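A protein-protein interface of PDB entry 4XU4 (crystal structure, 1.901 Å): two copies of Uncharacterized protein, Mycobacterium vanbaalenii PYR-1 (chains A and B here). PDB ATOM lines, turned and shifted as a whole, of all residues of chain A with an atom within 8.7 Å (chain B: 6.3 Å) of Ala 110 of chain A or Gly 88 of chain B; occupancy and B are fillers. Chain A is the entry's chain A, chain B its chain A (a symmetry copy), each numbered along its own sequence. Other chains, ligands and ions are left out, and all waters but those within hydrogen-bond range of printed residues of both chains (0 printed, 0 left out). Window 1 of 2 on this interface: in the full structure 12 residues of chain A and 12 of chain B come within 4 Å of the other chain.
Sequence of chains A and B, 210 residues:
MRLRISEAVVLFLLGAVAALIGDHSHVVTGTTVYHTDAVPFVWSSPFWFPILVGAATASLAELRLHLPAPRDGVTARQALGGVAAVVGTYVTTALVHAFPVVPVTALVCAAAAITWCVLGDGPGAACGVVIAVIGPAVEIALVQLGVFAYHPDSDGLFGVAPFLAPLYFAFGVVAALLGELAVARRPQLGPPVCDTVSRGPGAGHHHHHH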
ATOM      1  N   THR A  89      14.626 -10.338 -29.155  1.00  0.00           N
ATOM      2  CA  THR A  89      15.691 -11.101 -28.504  1.00  0.00           C
ATOM      3  C   THR A  89      16.802 -10.182 -28.005  1.00  0.00           C
ATOM      4  O   THR A  89      17.330 -10.361 -26.914  1.00  0.00           O
ATOM      5  CB  THR A  89      16.287 -12.154 -29.460  1.00  0.00           C
ATOM      6  OG1 THR A  89      15.237 -13.020 -29.918  1.00  0.00           O
ATOM      7  CG2 THR A  89      17.362 -12.981 -28.759  1.00  0.00           C
ATOM      8  N   VAL A 102      24.264 -19.733 -17.977  1.00  0.00           N
ATOM      9  CA  VAL A 102      23.658 -20.862 -18.684  1.00  0.00           C
ATOM     10  C   VAL A 102      22.188 -20.627 -19.055  1.00  0.00           C
ATOM     11  O   VAL A 102      21.846 -20.731 -20.223  1.00  0.00           O
ATOM     12  CB  VAL A 102      23.840 -22.213 -17.946  1.00  0.00           C
ATOM     13  CG1 VAL A 102      22.959 -23.295 -18.592  1.00  0.00           C
ATOM     14  CG2 VAL A 102      25.299 -22.631 -17.975  1.00  0.00           C
ATOM     15  N   PRO A 103      21.321 -20.312 -18.076  1.00  0.00           N
ATOM     16  CA  PRO A 103      19.946 -20.081 -18.528  1.00  0.00           C
ATOM     17  C   PRO A 103      19.817 -18.901 -19.497  1.00  0.00           C
ATOM     18  O   PRO A 103      19.041 -19.000 -20.446  1.00  0.00           O
ATOM     19  CB  PRO A 103      19.172 -19.817 -17.229  1.00  0.00           C
ATOM     20  CG  PRO A 103      20.226 -19.473 -16.202  1.00  0.00           C
ATOM     21  CD  PRO A 103      21.446 -20.235 -16.604  1.00  0.00           C
ATOM     22  N   VAL A 104      20.566 -17.822 -19.277  1.00  0.00           N
ATOM     23  CA  VAL A 104      20.516 -16.678 -20.195  1.00  0.00           C
ATOM     24  C   VAL A 104      20.931 -17.070 -21.607  1.00  0.00           C
ATOM     25  O   VAL A 104      20.238 -16.772 -22.580  1.00  0.00           O
ATOM     26  CB  VAL A 104      21.411 -15.514 -19.716  1.00  0.00           C
ATOM     27  CG1 VAL A 104      21.562 -14.475 -20.820  1.00  0.00           C
ATOM     28  CG2 VAL A 104      20.814 -14.885 -18.456  1.00  0.00           C
ATOM     29  N   THR A 105      22.070 -17.740 -21.727  1.00  0.00           N
ATOM     30  CA  THR A 105      22.548 -18.140 -23.041  1.00  0.00           C
ATOM     31  C   THR A 105      21.616 -19.178 -23.689  1.00  0.00           C
ATOM     32  O   THR A 105      21.359 -19.115 -24.889  1.00  0.00           O
ATOM     33  CB  THR A 105      23.976 -18.686 -22.964  1.00  0.00           C
ATOM     34  OG1 THR A 105      24.781 -17.780 -22.198  1.00  0.00           O
ATOM     35  CG2 THR A 105      24.559 -18.840 -24.358  1.00  0.00           C
ATOM     36  N   ALA A 106      21.101 -20.113 -22.894  1.00  0.00           N
ATOM     37  CA  ALA A 106      20.158 -21.114 -23.427  1.00  0.00           C
ATOM     38  C   ALA A 106      18.885 -20.465 -23.972  1.00  0.00           C
ATOM     39  O   ALA A 106      18.345 -20.901 -24.996  1.00  0.00           O
ATOM     40  CB  ALA A 106      19.811 -22.150 -22.362  1.00  0.00           C
ATOM     41  N   LEU A 107      18.406 -19.423 -23.295  1.00  0.00           N
ATOM     42  CA  LEU A 107      17.183 -18.745 -23.723  1.00  0.00           C
ATOM     43  C   LEU A 107      17.391 -18.086 -25.083  1.00  0.00           C
ATOM     44  O   LEU A 107      16.548 -18.189 -25.968  1.00  0.00           O
ATOM     45  CB  LEU A 107      16.750 -17.701 -22.684  1.00  0.00           C
ATOM     46  CG  LEU A 107      15.568 -16.808 -23.079  1.00  0.00           C
ATOM     47  CD1 LEU A 107      14.317 -17.652 -23.294  1.00  0.00           C
ATOM     48  CD2 LEU A 107      15.305 -15.734 -22.007  1.00  0.00           C
ATOM     49  N   VAL A 108      18.534 -17.431 -25.253  1.00  0.00           N
ATOM     50  CA  VAL A 108      18.846 -16.783 -26.521  1.00  0.00           C
ATOM     51  C   VAL A 108      19.069 -17.810 -27.640  1.00  0.00           C
ATOM     52  O   VAL A 108      18.640 -17.600 -28.773  1.00  0.00           O
ATOM     53  CB  VAL A 108      20.060 -15.834 -26.382  1.00  0.00           C
ATOM     54  CG1 VAL A 108      20.312 -15.087 -27.705  1.00  0.00           C
ATOM     55  CG2 VAL A 108      19.793 -14.832 -25.268  1.00  0.00           C
ATOM     56  N   CYS A 109      19.720 -18.925 -27.319  1.00  0.00           N
ATOM     57  CA  CYS A 109      19.872 -20.023 -28.283  1.00  0.00           C
ATOM     58  C   CYS A 109      18.520 -20.577 -28.721  1.00  0.00           C
ATOM     59  O   CYS A 109      18.334 -20.927 -29.888  1.00  0.00           O
ATOM     60  CB  CYS A 109      20.671 -21.183 -27.686  1.00  0.00           C
ATOM     61  SG  CYS A 109      22.440 -20.915 -27.509  1.00  0.00           S
ATOM     62  N   ALA A 110      17.592 -20.689 -27.777  1.00  0.00           N
ATOM     63  CA  ALA A 110      16.243 -21.164 -28.094  1.00  0.00           C
ATOM     64  C   ALA A 110      15.545 -20.187 -29.028  1.00  0.00           C
ATOM     65  O   ALA A 110      14.919 -20.587 -30.000  1.00  0.00           O
ATOM     66  CB  ALA A 110      15.429 -21.351 -26.820  1.00  0.00           C
ATOM     67  N   ALA A 111      15.658 -18.893 -28.734  1.00  0.00           N
ATOM     68  CA  ALA A 111      15.043 -17.875 -29.590  1.00  0.00           C
ATOM     69  C   ALA A 111      15.618 -17.929 -31.005  1.00  0.00           C
ATOM     70  O   ALA A 111      14.886 -17.813 -31.994  1.00  0.00           O
ATOM     71  CB  ALA A 111      15.232 -16.486 -28.978  1.00  0.00           C
ATOM     72  N   ALA A 112      16.928 -18.125 -31.100  1.00  0.00           N
ATOM     73  CA  ALA A 112      17.603 -18.162 -32.394  1.00  0.00           C
ATOM     74  C   ALA A 112      17.197 -19.396 -33.199  1.00  0.00           C
ATOM     75  O   ALA A 112      16.993 -19.323 -34.421  1.00  0.00           O
ATOM     76  CB  ALA A 112      19.112 -18.142 -32.189  1.00  0.00           C
ATOM     77  N   ALA A 113      17.089 -20.532 -32.516  1.00  0.00           N
ATOM     78  CA  ALA A 113      16.696 -21.776 -33.184  1.00  0.00           C
ATOM     79  C   ALA A 113      15.271 -21.660 -33.703  1.00  0.00           C
ATOM     80  O   ALA A 113      14.976 -22.059 -34.831  1.00  0.00           O
ATOM     81  CB  ALA A 113      16.835 -22.962 -32.244  1.00  0.00           C
ATOM     82  N   ILE A 114      14.381 -21.101 -32.891  1.00  0.00           N
ATOM     83  CA  ILE A 114      12.993 -20.941 -33.324  1.00  0.00           C
ATOM     84  C   ILE A 114      12.894 -19.975 -34.510  1.00  0.00           C
ATOM     85  O   ILE A 114      12.140 -20.217 -35.451  1.00  0.00           O
ATOM     86  CB  ILE A 114      12.096 -20.481 -32.158  1.00  0.00           C
ATOM     87  CG1 ILE A 114      11.928 -21.626 -31.153  1.00  0.00           C
ATOM     88  CG2 ILE A 114      10.726 -20.061 -32.658  1.00  0.00           C
ATOM     89  CD1 ILE A 114      11.293 -21.195 -29.843  1.00  0.00           C
ATOM     90  N   THR A 115      13.668 -18.892 -34.469  1.00  0.00           N
ATOM     91  CA  THR A 115      13.712 -17.945 -35.593  1.00  0.00           C
ATOM     92  C   THR A 115      14.139 -18.661 -36.874  1.00  0.00           C
ATOM     93  O   THR A 115      13.521 -18.495 -37.928  1.00  0.00           O
ATOM     94  CB  THR A 115      14.682 -16.769 -35.308  1.00  0.00           C
ATOM     95  OG1 THR A 115      14.293 -16.121 -34.092  1.00  0.00           O
ATOM     96  CG2 THR A 115      14.667 -15.753 -36.462  1.00  0.00           C
ATOM     97  N   TRP A 116      15.185 -19.480 -36.783  1.00  0.00           N
ATOM     98  CA  TRP A 116      15.609 -20.249 -37.956  1.00  0.00           C
ATOM     99  C   TRP A 116      14.514 -21.228 -38.398  1.00  0.00           C
ATOM    100  O   TRP A 116      14.213 -21.355 -39.595  1.00  0.00           O
ATOM    101  CB  TRP A 116      16.924 -21.016 -37.721  1.00  0.00           C
ATOM    102  CG  TRP A 116      17.297 -21.747 -38.973  1.00  0.00           C
ATOM    103  CD1 TRP A 116      18.007 -21.251 -40.033  1.00  0.00           C
ATOM    104  CD2 TRP A 116      16.907 -23.071 -39.336  1.00  0.00           C
ATOM    105  NE1 TRP A 116      18.094 -22.201 -41.033  1.00  0.00           N
ATOM    106  CE2 TRP A 116      17.418 -23.342 -40.626  1.00  0.00           C
ATOM    107  CE3 TRP A 116      16.161 -24.082 -38.696  1.00  0.00           C
ATOM    108  CZ2 TRP A 116      17.234 -24.553 -41.289  1.00  0.00           C
ATOM    109  CZ3 TRP A 116      15.966 -25.297 -39.353  1.00  0.00           C
ATOM    110  CH2 TRP A 116      16.502 -25.520 -40.634  1.00  0.00           C
ATOM    111  N   CYS A 117      13.924 -21.935 -37.439  1.00  0.00           N
ATOM    112  CA  CYS A 117      12.896 -22.922 -37.778  1.00  0.00           C
ATOM    113  C   CYS A 117      11.740 -22.304 -38.554  1.00  0.00           C
ATOM    114  O   CYS A 117      11.227 -22.902 -39.501  1.00  0.00           O
ATOM    115  CB  CYS A 117      12.363 -23.625 -36.524  1.00  0.00           C
ATOM    116  SG  CYS A 117      13.541 -24.733 -35.770  1.00  0.00           S
ATOM    117  N   PRO A 166      24.400 -16.729 -30.312  1.00  0.00           N
ATOM    118  CA  PRO A 166      23.093 -16.970 -30.946  1.00  0.00           C
ATOM    119  C   PRO A 166      22.381 -15.683 -31.372  1.00  0.00           C
ATOM    120  O   PRO A 166      21.579 -15.724 -32.298  1.00  0.00           O
ATOM    121  CB  PRO A 166      22.292 -17.700 -29.854  1.00  0.00           C
ATOM    122  CG  PRO A 166      22.970 -17.314 -28.559  1.00  0.00           C
ATOM    123  CD  PRO A 166      24.422 -17.171 -28.903  1.00  0.00           C
ATOM    124  N   LEU A 167      22.649 -14.561 -30.706  1.00  0.00           N
ATOM    125  CA  LEU A 167      22.031 -13.302 -31.125  1.00  0.00           C
ATOM    126  C   LEU A 167      22.495 -12.927 -32.527  1.00  0.00           C
ATOM    127  O   LEU A 167      21.675 -12.608 -33.389  1.00  0.00           O
ATOM    128  CB  LEU A 167      22.318 -12.165 -30.129  1.00  0.00           C
ATOM    129  CG  LEU A 167      21.804 -10.763 -30.488  1.00  0.00           C
ATOM    130  CD1 LEU A 167      20.304 -10.784 -30.707  1.00  0.00           C
ATOM    131  CD2 LEU A 167      22.177  -9.746 -29.381  1.00  0.00           C
ATOM    132  N   ALA A 170      21.002 -15.340 -35.241  1.00  0.00           N
ATOM    133  CA  ALA A 170      19.628 -14.990 -35.608  1.00  0.00           C
ATOM    134  C   ALA A 170      19.600 -13.748 -36.498  1.00  0.00           C
ATOM    135  O   ALA A 170      18.820 -13.674 -37.444  1.00  0.00           O
ATOM    136  CB  ALA A 170      18.773 -14.781 -34.342  1.00  0.00           C
ATOM    137  N   VAL B  83      11.790 -28.669 -29.442  1.00  0.00           N
ATOM    138  CA  VAL B  83      12.781 -28.831 -28.389  1.00  0.00           C
ATOM    139  C   VAL B  83      13.227 -27.455 -27.890  1.00  0.00           C
ATOM    140  O   VAL B  83      13.374 -27.233 -26.688  1.00  0.00           O
ATOM    141  CB  VAL B  83      13.982 -29.664 -28.872  1.00  0.00           C
ATOM    142  CG1 VAL B  83      15.108 -29.628 -27.842  1.00  0.00           C
ATOM    143  CG2 VAL B  83      13.536 -31.103 -29.126  1.00  0.00           C
ATOM    144  N   ALA B  84      13.414 -26.524 -28.823  1.00  0.00           N
ATOM    145  CA  ALA B  84      13.836 -25.175 -28.447  1.00  0.00           C
ATOM    146  C   ALA B  84      12.759 -24.499 -27.588  1.00  0.00           C
ATOM    147  O   ALA B  84      13.064 -23.806 -26.609  1.00  0.00           O
ATOM    148  CB  ALA B  84      14.149 -24.354 -29.696  1.00  0.00           C
ATOM    149  N   ALA B  85      11.493 -24.738 -27.920  1.00  0.00           N
ATOM    150  CA  ALA B  85      10.398 -24.115 -27.173  1.00  0.00           C
ATOM    151  C   ALA B  85      10.362 -24.639 -25.739  1.00  0.00           C
ATOM    152  O   ALA B  85      10.184 -23.876 -24.790  1.00  0.00           O
ATOM    153  CB  ALA B  85       9.058 -24.362 -27.866  1.00  0.00           C
ATOM    154  N   VAL B  86      10.559 -25.941 -25.583  1.00  0.00           N
ATOM    155  CA  VAL B  86      10.548 -26.534 -24.246  1.00  0.00           C
ATOM    156  C   VAL B  86      11.777 -26.123 -23.432  1.00  0.00           C
ATOM    157  O   VAL B  86      11.658 -25.773 -22.269  1.00  0.00           O
ATOM    158  CB  VAL B  86      10.420 -28.072 -24.304  1.00  0.00           C
ATOM    159  CG1 VAL B  86      10.586 -28.673 -22.906  1.00  0.00           C
ATOM    160  CG2 VAL B  86       9.063 -28.445 -24.878  1.00  0.00           C
ATOM    161  N   VAL B  87      12.944 -26.130 -24.057  1.00  0.00           N
ATOM    162  CA  VAL B  87      14.152 -25.673 -23.375  1.00  0.00           C
ATOM    163  C   VAL B  87      14.039 -24.195 -22.988  1.00  0.00           C
ATOM    164  O   VAL B  87      14.333 -23.824 -21.857  1.00  0.00           O
ATOM    165  CB  VAL B  87      15.402 -25.896 -24.244  1.00  0.00           C
ATOM    166  CG1 VAL B  87      16.589 -25.123 -23.685  1.00  0.00           C
ATOM    167  CG2 VAL B  87      15.724 -27.378 -24.301  1.00  0.00           C
ATOM    168  N   GLY B  88      13.584 -23.364 -23.921  1.00  0.00           N
ATOM    169  CA  GLY B  88      13.383 -21.950 -23.645  1.00  0.00           C
ATOM    170  C   GLY B  88      12.417 -21.698 -22.505  1.00  0.00           C
ATOM    171  O   GLY B  88      12.653 -20.835 -21.652  1.00  0.00           O
ATOM    172  N   THR B  89      11.326 -22.458 -22.471  1.00  0.00           N
ATOM    173  CA  THR B  89      10.345 -22.309 -21.396  1.00  0.00           C
ATOM    174  C   THR B  89      10.912 -22.785 -20.062  1.00  0.00           C
ATOM    175  O   THR B  89      10.703 -22.163 -19.026  1.00  0.00           O
ATOM    176  CB  THR B  89       9.051 -23.088 -21.710  1.00  0.00           C
ATOM    177  OG1 THR B  89       8.519 -22.629 -22.963  1.00  0.00           O
ATOM    178  CG2 THR B  89       8.013 -22.889 -20.609  1.00  0.00           C
ATOM    179  N   TYR B  90      11.627 -23.903 -20.101  1.00  0.00           N
ATOM    180  CA  TYR B  90      12.246 -24.479 -18.901  1.00  0.00           C
ATOM    181  C   TYR B  90      13.195 -23.453 -18.265  1.00  0.00           C
ATOM    182  O   TYR B  90      13.085 -23.142 -17.067  1.00  0.00           O
ATOM    183  CB  TYR B  90      13.010 -25.736 -19.329  1.00  0.00           C
ATOM    184  CG  TYR B  90      13.400 -26.729 -18.249  1.00  0.00           C
ATOM    185  CD1 TYR B  90      13.453 -26.373 -16.904  1.00  0.00           C
ATOM    186  CD2 TYR B  90      13.756 -28.023 -18.597  1.00  0.00           C
ATOM    187  CE1 TYR B  90      13.832 -27.300 -15.937  1.00  0.00           C
ATOM    188  CE2 TYR B  90      14.132 -28.946 -17.635  1.00  0.00           C
ATOM    189  CZ  TYR B  90      14.171 -28.580 -16.317  1.00  0.00           C
ATOM    190  OH  TYR B  90      14.552 -29.510 -15.372  1.00  0.00           O
ATOM    191  N   VAL B  91      14.114 -22.898 -19.055  1.00  0.00           N
ATOM    192  CA  VAL B  91      15.072 -21.946 -18.477  1.00  0.00           C
ATOM    193  C   VAL B  91      14.399 -20.636 -18.063  1.00  0.00           C
ATOM    194  O   VAL B  91      14.836 -19.993 -17.118  1.00  0.00           O
ATOM    195  CB  VAL B  91      16.314 -21.693 -19.381  1.00  0.00           C
ATOM    196  CG1 VAL B  91      17.053 -23.016 -19.649  1.00  0.00           C
ATOM    197  CG2 VAL B  91      15.920 -21.012 -20.698  1.00  0.00           C
ATOM    198  N   THR B  92      13.327 -20.251 -18.752  1.00  0.00           N
ATOM    199  CA  THR B  92      12.581 -19.051 -18.356  1.00  0.00           C
ATOM    200  C   THR B  92      11.988 -19.205 -16.958  1.00  0.00           C
ATOM    201  O   THR B  92      11.976 -18.248 -16.177  1.00  0.00           O
ATOM    202  CB  THR B  92      11.444 -18.706 -19.357  1.00  0.00           C
ATOM    203  OG1 THR B  92      12.010 -18.432 -20.646  1.00  0.00           O
ATOM    204  CG2 THR B  92      10.654 -17.469 -18.887  1.00  0.00           C
ATOM    205  N   THR B  93      11.498 -20.401 -16.628  1.00  0.00           N
ATOM    206  CA  THR B  93      10.956 -20.602 -15.285  1.00  0.00           C
ATOM    207  C   THR B  93      12.032 -20.370 -14.233  1.00  0.00           C
ATOM    208  O   THR B  93      11.735 -19.891 -13.145  1.00  0.00           O
ATOM    209  CB  THR B  93      10.301 -21.984 -15.066  1.00  0.00           C
ATOM    210  OG1 THR B  93      11.285 -23.024 -15.171  1.00  0.00           O
ATOM    211  CG2 THR B  93       9.166 -22.202 -16.074  1.00  0.00           C
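The side-chain sulfur of Cys 117 of chain A lies within hydrogen-bond range of the backbone carbonyl oxygen of Ala 113 of chain A, 3.2 Å away.
The side-chain hydroxyl (OG1) of Thr 92 of chain B sits at hydrogen-bond distance from the backbone carbonyl oxygen (O) of Gly 88 of chain B, at 2.7 Å.
Pro 103 of chain A touches Val 91 of chain B.
CG1 of Val 91 of chain B touches CB of Ala 106 of chain A (3.96 Å).
Gly 88 of chain B touches Leu 107 of chain A.
Leu 107 of chain A touches Val 91 of chain B.
Thr 92 of chain B touches Leu 107 of chain A (OG1 to CD1, 3.6 Å).
Ala 84 of chain B touches Ala 110 of chain A.
Ala 110 of chain A touches Gly 88 of chain B.
Ala 84 of chain B touches Ala 113 of chain A (CB to CB, 3.96 Å).
Ala 84 of chain B touches Ile 114 of chain A (CB to CG1, 3.8 Å).
Of chain A, only Leu 107 (3.9 Å) and Ala 110 (3.8 Å) come within 4 Å of Gly 88 of chain B.
Val 87 of chain B touches none of the printed residues of chain A.
Of the printed residues of chain B, Ala 106 of chain A touches Val 91.
Of the printed residues of chain B, Ile 114 of chain A touches Ala 84.
Ala 170 of chain A touches none of the printed residues of chain B.
Hydrophobic or aromatic side chains of chain B within 4 Å of the printed part of chain A: Ala 84 and Val 91.
Of the 20 printed residues of chain A, 6 touch a printed residue of chain B.
Among the printed residues, 9 pairs touch across the chains.
Among the printed residues, no Asp or Glu carboxylate lies within 4 Å of a Lys or Arg side-chain nitrogen of the other chain.
1 position is printed for both chains.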
